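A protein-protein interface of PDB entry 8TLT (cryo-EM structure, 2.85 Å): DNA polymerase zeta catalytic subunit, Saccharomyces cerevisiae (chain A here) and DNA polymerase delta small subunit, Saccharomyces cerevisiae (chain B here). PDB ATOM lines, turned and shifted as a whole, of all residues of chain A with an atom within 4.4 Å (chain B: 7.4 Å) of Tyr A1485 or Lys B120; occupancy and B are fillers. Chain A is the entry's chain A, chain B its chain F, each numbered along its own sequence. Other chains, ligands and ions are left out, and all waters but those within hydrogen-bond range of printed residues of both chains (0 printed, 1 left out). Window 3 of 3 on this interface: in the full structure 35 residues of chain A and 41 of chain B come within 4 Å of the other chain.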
ATOM      1  N   ARG A1481       3.522  14.585  -1.862  1.00  0.00           N
ATOM      2  CA  ARG A1481       3.851  15.521  -0.790  1.00  0.00           C
ATOM      3  C   ARG A1481       3.357  15.011   0.558  1.00  0.00           C
ATOM      4  O   ARG A1481       4.084  15.068   1.562  1.00  0.00           O
ATOM      5  CB  ARG A1481       3.249  16.887  -1.110  1.00  0.00           C
ATOM      6  CG  ARG A1481       3.672  18.009  -0.194  1.00  0.00           C
ATOM      7  CD  ARG A1481       2.954  19.295  -0.571  1.00  0.00           C
ATOM      8  NE  ARG A1481       2.930  19.492  -2.015  1.00  0.00           N
ATOM      9  CZ  ARG A1481       1.826  19.657  -2.733  1.00  0.00           C
ATOM     10  NH1 ARG A1481       0.631  19.664  -2.169  1.00  0.00           N
ATOM     11  NH2 ARG A1481       1.927  19.820  -4.049  1.00  0.00           N
ATOM     12  N   THR A1482       2.130  14.487   0.599  1.00  0.00           N
ATOM     13  CA  THR A1482       1.616  13.916   1.839  1.00  0.00           C
ATOM     14  C   THR A1482       2.452  12.722   2.282  1.00  0.00           C
ATOM     15  O   THR A1482       2.694  12.535   3.480  1.00  0.00           O
ATOM     16  CB  THR A1482       0.152  13.513   1.669  1.00  0.00           C
ATOM     17  N   CYS A1483       2.899  11.900   1.330  1.00  0.00           N
ATOM     18  CA  CYS A1483       3.749  10.762   1.672  1.00  0.00           C
ATOM     19  C   CYS A1483       5.092  11.219   2.232  1.00  0.00           C
ATOM     20  O   CYS A1483       5.564  10.691   3.245  1.00  0.00           O
ATOM     21  CB  CYS A1483       3.951   9.872   0.446  1.00  0.00           C
ATOM     22  SG  CYS A1483       4.937   8.394   0.750  1.00  0.00           S
ATOM     23  N   SER A1484       5.722  12.204   1.588  1.00  0.00           N
ATOM     24  CA  SER A1484       7.020  12.701   2.031  1.00  0.00           C
ATOM     25  C   SER A1484       6.938  13.493   3.327  1.00  0.00           C
ATOM     26  O   SER A1484       7.980  13.748   3.945  1.00  0.00           O
ATOM     27  CB  SER A1484       7.651  13.567   0.942  1.00  0.00           C
ATOM     28  N   TYR A1485       5.734  13.889   3.746  1.00  0.00           N
ATOM     29  CA  TYR A1485       5.579  14.528   5.049  1.00  0.00           C
ATOM     30  C   TYR A1485       6.065  13.640   6.187  1.00  0.00           C
ATOM     31  O   TYR A1485       6.386  14.153   7.264  1.00  0.00           O
ATOM     32  CB  TYR A1485       4.113  14.905   5.272  1.00  0.00           C
ATOM     33  CG  TYR A1485       3.847  15.689   6.540  1.00  0.00           C
ATOM     34  CD1 TYR A1485       3.975  17.069   6.563  1.00  0.00           C
ATOM     35  CD2 TYR A1485       3.458  15.047   7.708  1.00  0.00           C
ATOM     36  CE1 TYR A1485       3.730  17.788   7.715  1.00  0.00           C
ATOM     37  CE2 TYR A1485       3.212  15.759   8.863  1.00  0.00           C
ATOM     38  CZ  TYR A1485       3.349  17.128   8.861  1.00  0.00           C
ATOM     39  OH  TYR A1485       3.104  17.843  10.010  1.00  0.00           O
ATOM     40  N   ARG A1486       6.132  12.322   5.972  1.00  0.00           N
ATOM     41  CA  ARG A1486       6.617  11.417   7.010  1.00  0.00           C
ATOM     42  C   ARG A1486       8.057  11.734   7.394  1.00  0.00           C
ATOM     43  O   ARG A1486       8.403  11.741   8.581  1.00  0.00           O
ATOM     44  CB  ARG A1486       6.497   9.970   6.533  1.00  0.00           C
ATOM     45  CG  ARG A1486       7.249   8.968   7.388  1.00  0.00           C
ATOM     46  CD  ARG A1486       7.465   7.660   6.646  1.00  0.00           C
ATOM     47  NE  ARG A1486       6.212   6.955   6.407  1.00  0.00           N
ATOM     48  CZ  ARG A1486       5.694   6.050   7.225  1.00  0.00           C
ATOM     49  NH1 ARG A1486       6.296   5.715   8.354  1.00  0.00           N
ATOM     50  NH2 ARG A1486       4.542   5.470   6.905  1.00  0.00           N
ATOM     51  N   TYR A1487       8.911  11.998   6.406  1.00  0.00           N
ATOM     52  CA  TYR A1487      10.294  12.372   6.669  1.00  0.00           C
ATOM     53  C   TYR A1487      10.443  13.871   6.893  1.00  0.00           C
ATOM     54  O   TYR A1487      11.034  14.297   7.890  1.00  0.00           O
ATOM     55  CB  TYR A1487      11.195  11.941   5.509  1.00  0.00           C
ATOM     56  CG  TYR A1487      11.216  10.461   5.231  1.00  0.00           C
ATOM     57  CD1 TYR A1487      11.018   9.538   6.245  1.00  0.00           C
ATOM     58  CD2 TYR A1487      11.444   9.986   3.950  1.00  0.00           C
ATOM     59  CE1 TYR A1487      11.040   8.184   5.987  1.00  0.00           C
ATOM     60  CE2 TYR A1487      11.468   8.637   3.684  1.00  0.00           C
ATOM     61  CZ  TYR A1487      11.266   7.740   4.705  1.00  0.00           C
ATOM     62  OH  TYR A1487      11.291   6.392   4.440  1.00  0.00           O
ATOM     63  N   THR A1488       9.915  14.680   5.972  1.00  0.00           N
ATOM     64  CA  THR A1488      10.159  16.118   6.022  1.00  0.00           C
ATOM     65  C   THR A1488       9.487  16.765   7.227  1.00  0.00           C
ATOM     66  O   THR A1488      10.061  17.662   7.854  1.00  0.00           O
ATOM     67  CB  THR A1488       9.684  16.778   4.729  1.00  0.00           C
ATOM     68  N   SER A1489       8.271  16.326   7.560  1.00  0.00           N
ATOM     69  CA  SER A1489       7.448  16.965   8.589  1.00  0.00           C
ATOM     70  C   SER A1489       7.226  18.443   8.283  1.00  0.00           C
ATOM     71  O   SER A1489       7.157  19.276   9.189  1.00  0.00           O
ATOM     72  CB  SER A1489       8.049  16.787   9.985  1.00  0.00           C
ATOM     73  OG  SER A1489       7.166  17.265  10.982  1.00  0.00           O
ATOM     74  N   ASP A1490       7.113  18.769   6.997  1.00  0.00           N
ATOM     75  CA  ASP A1490       6.922  20.132   6.527  1.00  0.00           C
ATOM     76  C   ASP A1490       5.840  20.123   5.458  1.00  0.00           C
ATOM     77  O   ASP A1490       5.630  19.115   4.781  1.00  0.00           O
ATOM     78  CB  ASP A1490       8.228  20.716   5.969  1.00  0.00           C
ATOM     79  CG  ASP A1490       8.142  22.204   5.712  1.00  0.00           C
ATOM     80  OD1 ASP A1490       7.765  22.949   6.640  1.00  0.00           O
ATOM     81  OD2 ASP A1490       8.458  22.631   4.582  1.00  0.00           O
ATOM     82  N   ASN A1495       9.577  20.828   0.936  1.00  0.00           N
ATOM     83  CA  ASN A1495       8.982  19.508   1.091  1.00  0.00           C
ATOM     84  C   ASN A1495       8.500  18.934  -0.231  1.00  0.00           C
ATOM     85  O   ASN A1495       8.557  17.716  -0.424  1.00  0.00           O
ATOM     86  CB  ASN A1495       7.812  19.562   2.078  1.00  0.00           C
ATOM     87  CG  ASN A1495       7.090  18.235   2.204  1.00  0.00           C
ATOM     88  OD1 ASN A1495       7.707  17.173   2.180  1.00  0.00           O
ATOM     89  ND2 ASN A1495       5.773  18.292   2.347  1.00  0.00           N
ATOM     90  N   TYR B 116       7.661  28.483  11.012  1.00  0.00           N
ATOM     91  CA  TYR B 116       7.402  27.062  10.819  1.00  0.00           C
ATOM     92  C   TYR B 116       6.137  26.664  11.571  1.00  0.00           C
ATOM     93  O   TYR B 116       5.952  27.051  12.729  1.00  0.00           O
ATOM     94  CB  TYR B 116       8.589  26.220  11.294  1.00  0.00           C
ATOM     95  CG  TYR B 116       8.377  24.730  11.156  1.00  0.00           C
ATOM     96  CD1 TYR B 116       8.473  24.109   9.920  1.00  0.00           C
ATOM     97  CD2 TYR B 116       8.078  23.945  12.261  1.00  0.00           C
ATOM     98  CE1 TYR B 116       8.278  22.749   9.787  1.00  0.00           C
ATOM     99  CE2 TYR B 116       7.880  22.584  12.137  1.00  0.00           C
ATOM    100  CZ  TYR B 116       7.981  21.991  10.898  1.00  0.00           C
ATOM    101  N   CYS B 117       5.275  25.893  10.910  1.00  0.00           N
ATOM    102  CA  CYS B 117       4.022  25.427  11.491  1.00  0.00           C
ATOM    103  C   CYS B 117       3.760  24.003  11.016  1.00  0.00           C
ATOM    104  O   CYS B 117       4.526  23.438  10.230  1.00  0.00           O
ATOM    105  CB  CYS B 117       2.860  26.358  11.124  1.00  0.00           C
ATOM    106  SG  CYS B 117       2.929  27.985  11.898  1.00  0.00           S
ATOM    107  N   GLU B 118       2.661  23.416  11.497  1.00  0.00           N
ATOM    108  CA  GLU B 118       2.350  22.028  11.164  1.00  0.00           C
ATOM    109  C   GLU B 118       1.676  21.915   9.800  1.00  0.00           C
ATOM    110  O   GLU B 118       2.226  21.310   8.874  1.00  0.00           O
ATOM    111  CB  GLU B 118       1.465  21.416  12.253  1.00  0.00           C
ATOM    112  N   MET B 119       0.481  22.495   9.663  1.00  0.00           N
ATOM    113  CA  MET B 119      -0.255  22.551   8.399  1.00  0.00           C
ATOM    114  C   MET B 119      -0.506  21.148   7.834  1.00  0.00           C
ATOM    115  O   MET B 119       0.025  20.751   6.796  1.00  0.00           O
ATOM    116  CB  MET B 119       0.474  23.435   7.381  1.00  0.00           C
ATOM    117  CG  MET B 119       0.705  24.853   7.855  1.00  0.00           C
ATOM    118  SD  MET B 119       1.067  25.999   6.513  1.00  0.00           S
ATOM    119  CE  MET B 119       0.741  24.984   5.078  1.00  0.00           C
ATOM    120  N   LYS B 120      -1.325  20.398   8.565  1.00  0.00           N
ATOM    121  CA  LYS B 120      -1.784  19.100   8.094  1.00  0.00           C
ATOM    122  C   LYS B 120      -2.947  19.264   7.121  1.00  0.00           C
ATOM    123  O   LYS B 120      -3.759  20.183   7.240  1.00  0.00           O
ATOM    124  CB  LYS B 120      -2.213  18.225   9.271  1.00  0.00           C
ATOM    125  CG  LYS B 120      -1.120  17.326   9.815  1.00  0.00           C
ATOM    126  CD  LYS B 120      -0.961  17.504  11.314  1.00  0.00           C
ATOM    127  CE  LYS B 120       0.066  16.538  11.877  1.00  0.00           C
ATOM    128  NZ  LYS B 120      -0.287  15.124  11.575  1.00  0.00           N
ATOM    129  N   TYR B 121      -3.019  18.359   6.148  1.00  0.00           N
ATOM    130  CA  TYR B 121      -4.117  18.377   5.192  1.00  0.00           C
ATOM    131  C   TYR B 121      -5.413  17.920   5.854  1.00  0.00           C
ATOM    132  O   TYR B 121      -5.412  17.103   6.778  1.00  0.00           O
ATOM    133  CB  TYR B 121      -3.807  17.478   3.996  1.00  0.00           C
ATOM    134  CG  TYR B 121      -3.183  18.193   2.818  1.00  0.00           C
ATOM    135  CD1 TYR B 121      -3.836  19.245   2.195  1.00  0.00           C
ATOM    136  CD2 TYR B 121      -1.944  17.809   2.325  1.00  0.00           C
ATOM    137  CE1 TYR B 121      -3.271  19.898   1.119  1.00  0.00           C
ATOM    138  CE2 TYR B 121      -1.372  18.457   1.249  1.00  0.00           C
ATOM    139  CZ  TYR B 121      -2.039  19.500   0.651  1.00  0.00           C
ATOM    140  OH  TYR B 121      -1.473  20.149  -0.421  1.00  0.00           O
ATOM    141  N   LYS B 122      -6.529  18.460   5.372  1.00  0.00           N
ATOM    142  CA  LYS B 122      -7.827  18.063   5.890  1.00  0.00           C
ATOM    143  C   LYS B 122      -8.169  16.644   5.434  1.00  0.00           C
ATOM    144  O   LYS B 122      -7.766  16.218   4.350  1.00  0.00           O
ATOM    145  CB  LYS B 122      -8.907  19.038   5.432  1.00  0.00           C
ATOM    146  CG  LYS B 122      -8.988  20.287   6.290  1.00  0.00           C
ATOM    147  CD  LYS B 122     -10.067  21.240   5.818  1.00  0.00           C
ATOM    148  CE  LYS B 122     -10.157  22.445   6.738  1.00  0.00           C
ATOM    149  NZ  LYS B 122     -11.112  23.467   6.236  1.00  0.00           N
ATOM    150  N   PRO B 123      -8.902  15.886   6.257  1.00  0.00           N
ATOM    151  CA  PRO B 123      -9.205  14.491   5.892  1.00  0.00           C
ATOM    152  C   PRO B 123      -9.993  14.350   4.602  1.00  0.00           C
ATOM    153  O   PRO B 123      -9.805  13.363   3.880  1.00  0.00           O
ATOM    154  CB  PRO B 123     -10.001  13.979   7.101  1.00  0.00           C
ATOM    155  CG  PRO B 123     -10.518  15.204   7.771  1.00  0.00           C
ATOM    156  CD  PRO B 123      -9.477  16.253   7.561  1.00  0.00           C
ATOM    157  N   LEU B 126      -7.516  14.399   1.752  1.00  0.00           N
ATOM    158  CA  LEU B 126      -6.822  13.122   1.633  1.00  0.00           C
ATOM    159  C   LEU B 126      -7.720  12.062   1.013  1.00  0.00           C
ATOM    160  O   LEU B 126      -7.277  11.285   0.161  1.00  0.00           O
ATOM    161  CB  LEU B 126      -6.322  12.667   3.003  1.00  0.00           C
ATOM    162  CG  LEU B 126      -5.289  13.565   3.681  1.00  0.00           C
ATOM    163  CD1 LEU B 126      -4.905  12.996   5.032  1.00  0.00           C
ATOM    164  CD2 LEU B 126      -4.066  13.728   2.799  1.00  0.00           C
ATOM    165  N   LEU B 139      -2.570   7.825   3.673  1.00  0.00           N
ATOM    166  CA  LEU B 139      -1.972   9.105   4.031  1.00  0.00           C
ATOM    167  C   LEU B 139      -2.329   9.517   5.454  1.00  0.00           C
ATOM    168  O   LEU B 139      -1.558  10.232   6.104  1.00  0.00           O
ATOM    169  CB  LEU B 139      -2.415  10.175   3.034  1.00  0.00           C
ATOM    170  CG  LEU B 139      -2.073   9.887   1.569  1.00  0.00           C
ATOM    171  CD1 LEU B 139      -2.431  11.068   0.686  1.00  0.00           C
ATOM    172  CD2 LEU B 139      -0.604   9.533   1.420  1.00  0.00           C
ATOM    173  N   THR B 140      -3.488   9.077   5.951  1.00  0.00           N
ATOM    174  CA  THR B 140      -3.834   9.326   7.345  1.00  0.00           C
ATOM    175  C   THR B 140      -2.830   8.667   8.281  1.00  0.00           C
ATOM    176  O   THR B 140      -2.423   9.262   9.287  1.00  0.00           O
ATOM    177  CB  THR B 140      -5.247   8.821   7.636  1.00  0.00           C
ATOM    178  N   SER B 142       0.245   8.052   7.502  1.00  0.00           N
ATOM    179  CA  SER B 142       1.466   8.838   7.359  1.00  0.00           C
ATOM    180  C   SER B 142       1.433  10.072   8.250  1.00  0.00           C
ATOM    181  O   SER B 142       2.444  10.430   8.866  1.00  0.00           O
ATOM    182  CB  SER B 142       1.666   9.240   5.898  1.00  0.00           C
ATOM    183  OG  SER B 142       3.026   9.534   5.631  1.00  0.00           O
ATOM    184  N   TYR B 143       0.282  10.744   8.322  1.00  0.00           N
ATOM    185  CA  TYR B 143       0.158  11.887   9.221  1.00  0.00           C
ATOM    186  C   TYR B 143       0.262  11.456  10.679  1.00  0.00           C
ATOM    187  O   TYR B 143       0.917  12.129  11.484  1.00  0.00           O
ATOM    188  CB  TYR B 143      -1.157  12.622   8.965  1.00  0.00           C
ATOM    189  CG  TYR B 143      -1.038  13.711   7.926  1.00  0.00           C
ATOM    190  CD1 TYR B 143       0.040  14.582   7.931  1.00  0.00           C
ATOM    191  CD2 TYR B 143      -1.999  13.864   6.937  1.00  0.00           C
ATOM    192  CE1 TYR B 143       0.159  15.576   6.983  1.00  0.00           C
ATOM    193  CE2 TYR B 143      -1.888  14.858   5.984  1.00  0.00           C
ATOM    194  CZ  TYR B 143      -0.806  15.710   6.014  1.00  0.00           C
ATOM    195  OH  TYR B 143      -0.684  16.703   5.071  1.00  0.00           O
ATOM    196  N   THR B 144      -0.371  10.338  11.030  1.00  0.00           N
ATOM    197  CA  THR B 144      -0.341   9.787  12.386  1.00  0.00           C
ATOM    198  C   THR B 144      -0.760  10.812  13.437  1.00  0.00           C
ATOM    199  O   THR B 144       0.072  11.314  14.192  1.00  0.00           O
ATOM    200  CB  THR B 144       1.058   9.243  12.747  1.00  0.00           C
ATOM    201  N   GLY B 149       1.412  15.527  16.585  1.00  0.00           N
ATOM    202  CA  GLY B 149       1.526  16.785  15.871  1.00  0.00           C
ATOM    203  C   GLY B 149       2.193  17.878  16.683  1.00  0.00           C
ATOM    204  O   GLY B 149       2.666  17.640  17.793  1.00  0.00           O
ATOM    205  N   SER B 150       2.235  19.084  16.120  1.00  0.00           N
ATOM    206  CA  SER B 150       2.839  20.236  16.777  1.00  0.00           C
ATOM    207  C   SER B 150       1.846  21.389  16.781  1.00  0.00           C
ATOM    208  O   SER B 150       1.285  21.732  15.736  1.00  0.00           O
ATOM    209  CB  SER B 150       4.137  20.656  16.078  1.00  0.00           C
ATOM    210  N   ILE B 370      -5.271  28.031   1.294  1.00  0.00           N
ATOM    211  CA  ILE B 370      -4.800  28.059   2.676  1.00  0.00           C
ATOM    212  C   ILE B 370      -5.820  27.401   3.594  1.00  0.00           C
ATOM    213  O   ILE B 370      -5.451  26.761   4.587  1.00  0.00           O
ATOM    214  CB  ILE B 370      -4.481  29.493   3.135  1.00  0.00           C
ATOM    215  CG1 ILE B 370      -5.517  30.476   2.605  1.00  0.00           C
ATOM    216  CG2 ILE B 370      -3.096  29.907   2.679  1.00  0.00           C
ATOM    217  N   LYS B 372      -7.637  24.845   3.102  1.00  0.00           N
ATOM    218  CA  LYS B 372      -7.703  23.395   2.983  1.00  0.00           C
ATOM    219  C   LYS B 372      -6.711  22.682   3.893  1.00  0.00           C
ATOM    220  O   LYS B 372      -6.673  21.448   3.900  1.00  0.00           O
ATOM    221  CB  LYS B 372      -7.485  22.973   1.527  1.00  0.00           C
ATOM    222  CG  LYS B 372      -6.035  22.833   1.112  1.00  0.00           C
ATOM    223  CD  LYS B 372      -5.909  21.962  -0.124  1.00  0.00           C
ATOM    224  CE  LYS B 372      -6.842  22.430  -1.225  1.00  0.00           C
ATOM    225  NZ  LYS B 372      -6.652  21.649  -2.476  1.00  0.00           N
ATOM    226  N   TYR B 373      -5.919  23.424   4.658  1.00  0.00           N
ATOM    227  CA  TYR B 373      -4.993  22.868   5.631  1.00  0.00           C
ATOM    228  C   TYR B 373      -5.590  22.943   7.031  1.00  0.00           C
ATOM    229  O   TYR B 373      -6.476  23.751   7.312  1.00  0.00           O
ATOM    230  CB  TYR B 373      -3.660  23.619   5.601  1.00  0.00           C
ATOM    231  CG  TYR B 373      -2.763  23.262   4.441  1.00  0.00           C
ATOM    232  CD1 TYR B 373      -2.131  22.030   4.379  1.00  0.00           C
ATOM    233  CD2 TYR B 373      -2.546  24.162   3.408  1.00  0.00           C
ATOM    234  CE1 TYR B 373      -1.309  21.704   3.322  1.00  0.00           C
ATOM    235  CE2 TYR B 373      -1.727  23.844   2.347  1.00  0.00           C
ATOM    236  CZ  TYR B 373      -1.111  22.615   2.309  1.00  0.00           C
ATOM    237  OH  TYR B 373      -0.293  22.297   1.250  1.00  0.00           O
ATOM    238  N   VAL B 374      -5.086  22.085   7.911  1.00  0.00           N
ATOM    239  CA  VAL B 374      -5.409  22.126   9.333  1.00  0.00           C
ATOM    240  C   VAL B 374      -4.179  22.659  10.051  1.00  0.00           C
ATOM    241  O   VAL B 374      -3.132  21.999  10.084  1.00  0.00           O
ATOM    242  CB  VAL B 374      -5.818  20.749   9.872  1.00  0.00           C
ATOM    243  CG1 VAL B 374      -5.766  20.736  11.390  1.00  0.00           C
ATOM    244  CG2 VAL B 374      -7.207  20.383   9.390  1.00  0.00           C
ATOM    245  N   ILE B 375      -4.293  23.850  10.620  1.00  0.00           N
ATOM    246  CA  ILE B 375      -3.193  24.515  11.303  1.00  0.00           C
ATOM    247  C   ILE B 375      -3.556  24.645  12.775  1.00  0.00           C
ATOM    248  O   ILE B 375      -4.319  25.530  13.163  1.00  0.00           O
ATOM    249  CB  ILE B 375      -2.891  25.891  10.681  1.00  0.00           C
ATOM    250  CG1 ILE B 375      -2.644  25.753   9.179  1.00  0.00           C
ATOM    251  CG2 ILE B 375      -1.688  26.525  11.353  1.00  0.00           C
ATOM    252  CD1 ILE B 375      -2.674  27.065   8.432  1.00  0.00           C
ATOM    253  N   PRO B 376      -3.020  23.770  13.638  1.00  0.00           N
ATOM    254  CA  PRO B 376      -3.346  23.791  15.070  1.00  0.00           C
ATOM    255  C   PRO B 376      -2.598  24.871  15.849  1.00  0.00           C
ATOM    256  O   PRO B 376      -2.056  24.623  16.926  1.00  0.00           O
ATOM    257  CB  PRO B 376      -2.950  22.384  15.525  1.00  0.00           C
ATOM    258  CG  PRO B 376      -1.826  22.016  14.626  1.00  0.00           C
ATOM    259  CD  PRO B 376      -2.070  22.695  13.304  1.00  0.00           C
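NH1 of Arg A1481 lies within hydrogen-bond range of OH of Tyr B121 (2.8 Å).
CB of Thr A1482 touches CD1 of Leu B139, 3.7 Å away.
O of Thr A1482 touches OG of Ser B142 (3.7 Å).
OG of Ser B142 touches O of Cys A1483, 3.7 Å away.
Tyr A1485 touches Glu B118.
Lys B120 touches Tyr A1485.
Tyr A1485 touches Tyr B143 (CD2 to CE1, 3.4 Å).
CB of Arg A1486 touches OG of Ser B142 (3.6 Å).
Tyr B116 touches Ser A1489.
Asp A1490 touches Tyr B116.
Printed residues of chain B within 4 Å of Arg A1481: Tyr B121 (2.8 Å).
Of the printed residues of chain B, Thr A1482 touches Leu B139 (3.7 Å) and Ser B142 (3.7 Å).
Of chain B, only Glu B118, Lys B120 and Tyr B143 come within 4 Å of Tyr A1485.
Of the printed residues of chain A, Tyr B116 touches Ser A1489 and Asp A1490.
Lys B120 touches one residue of chain A.
The nearest residue of chain B that does not touch Tyr A1485 is Met B119 (4.8 Å).
OH of Tyr B373 lies within hydrogen-bond range of OH of Tyr B121, 3.0 Å away.
N of Val B374 lies within hydrogen-bond range of O of Lys B120 (2.4 Å).
The backbone NH (N) of Tyr B121 is in hydrogen-bond range of the side-chain hydroxyl (OH) of Tyr B143 (3.1 Å).
The side-chain amide nitrogen (ND2) of Asn A1495 sits at hydrogen-bond distance from the backbone carbonyl oxygen (O) of Asp A1490.
The side-chain amino group (NZ) of Lys B120 sits at hydrogen-bond distance from the backbone carbonyl oxygen (O) of Tyr B143, 3.2 Å away.
Of the 22 printed residues of chain B, 7 touch a printed residue of chain A.
Along chain B the printed residues that touch a printed residue of chain A span positions 116 to 143.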
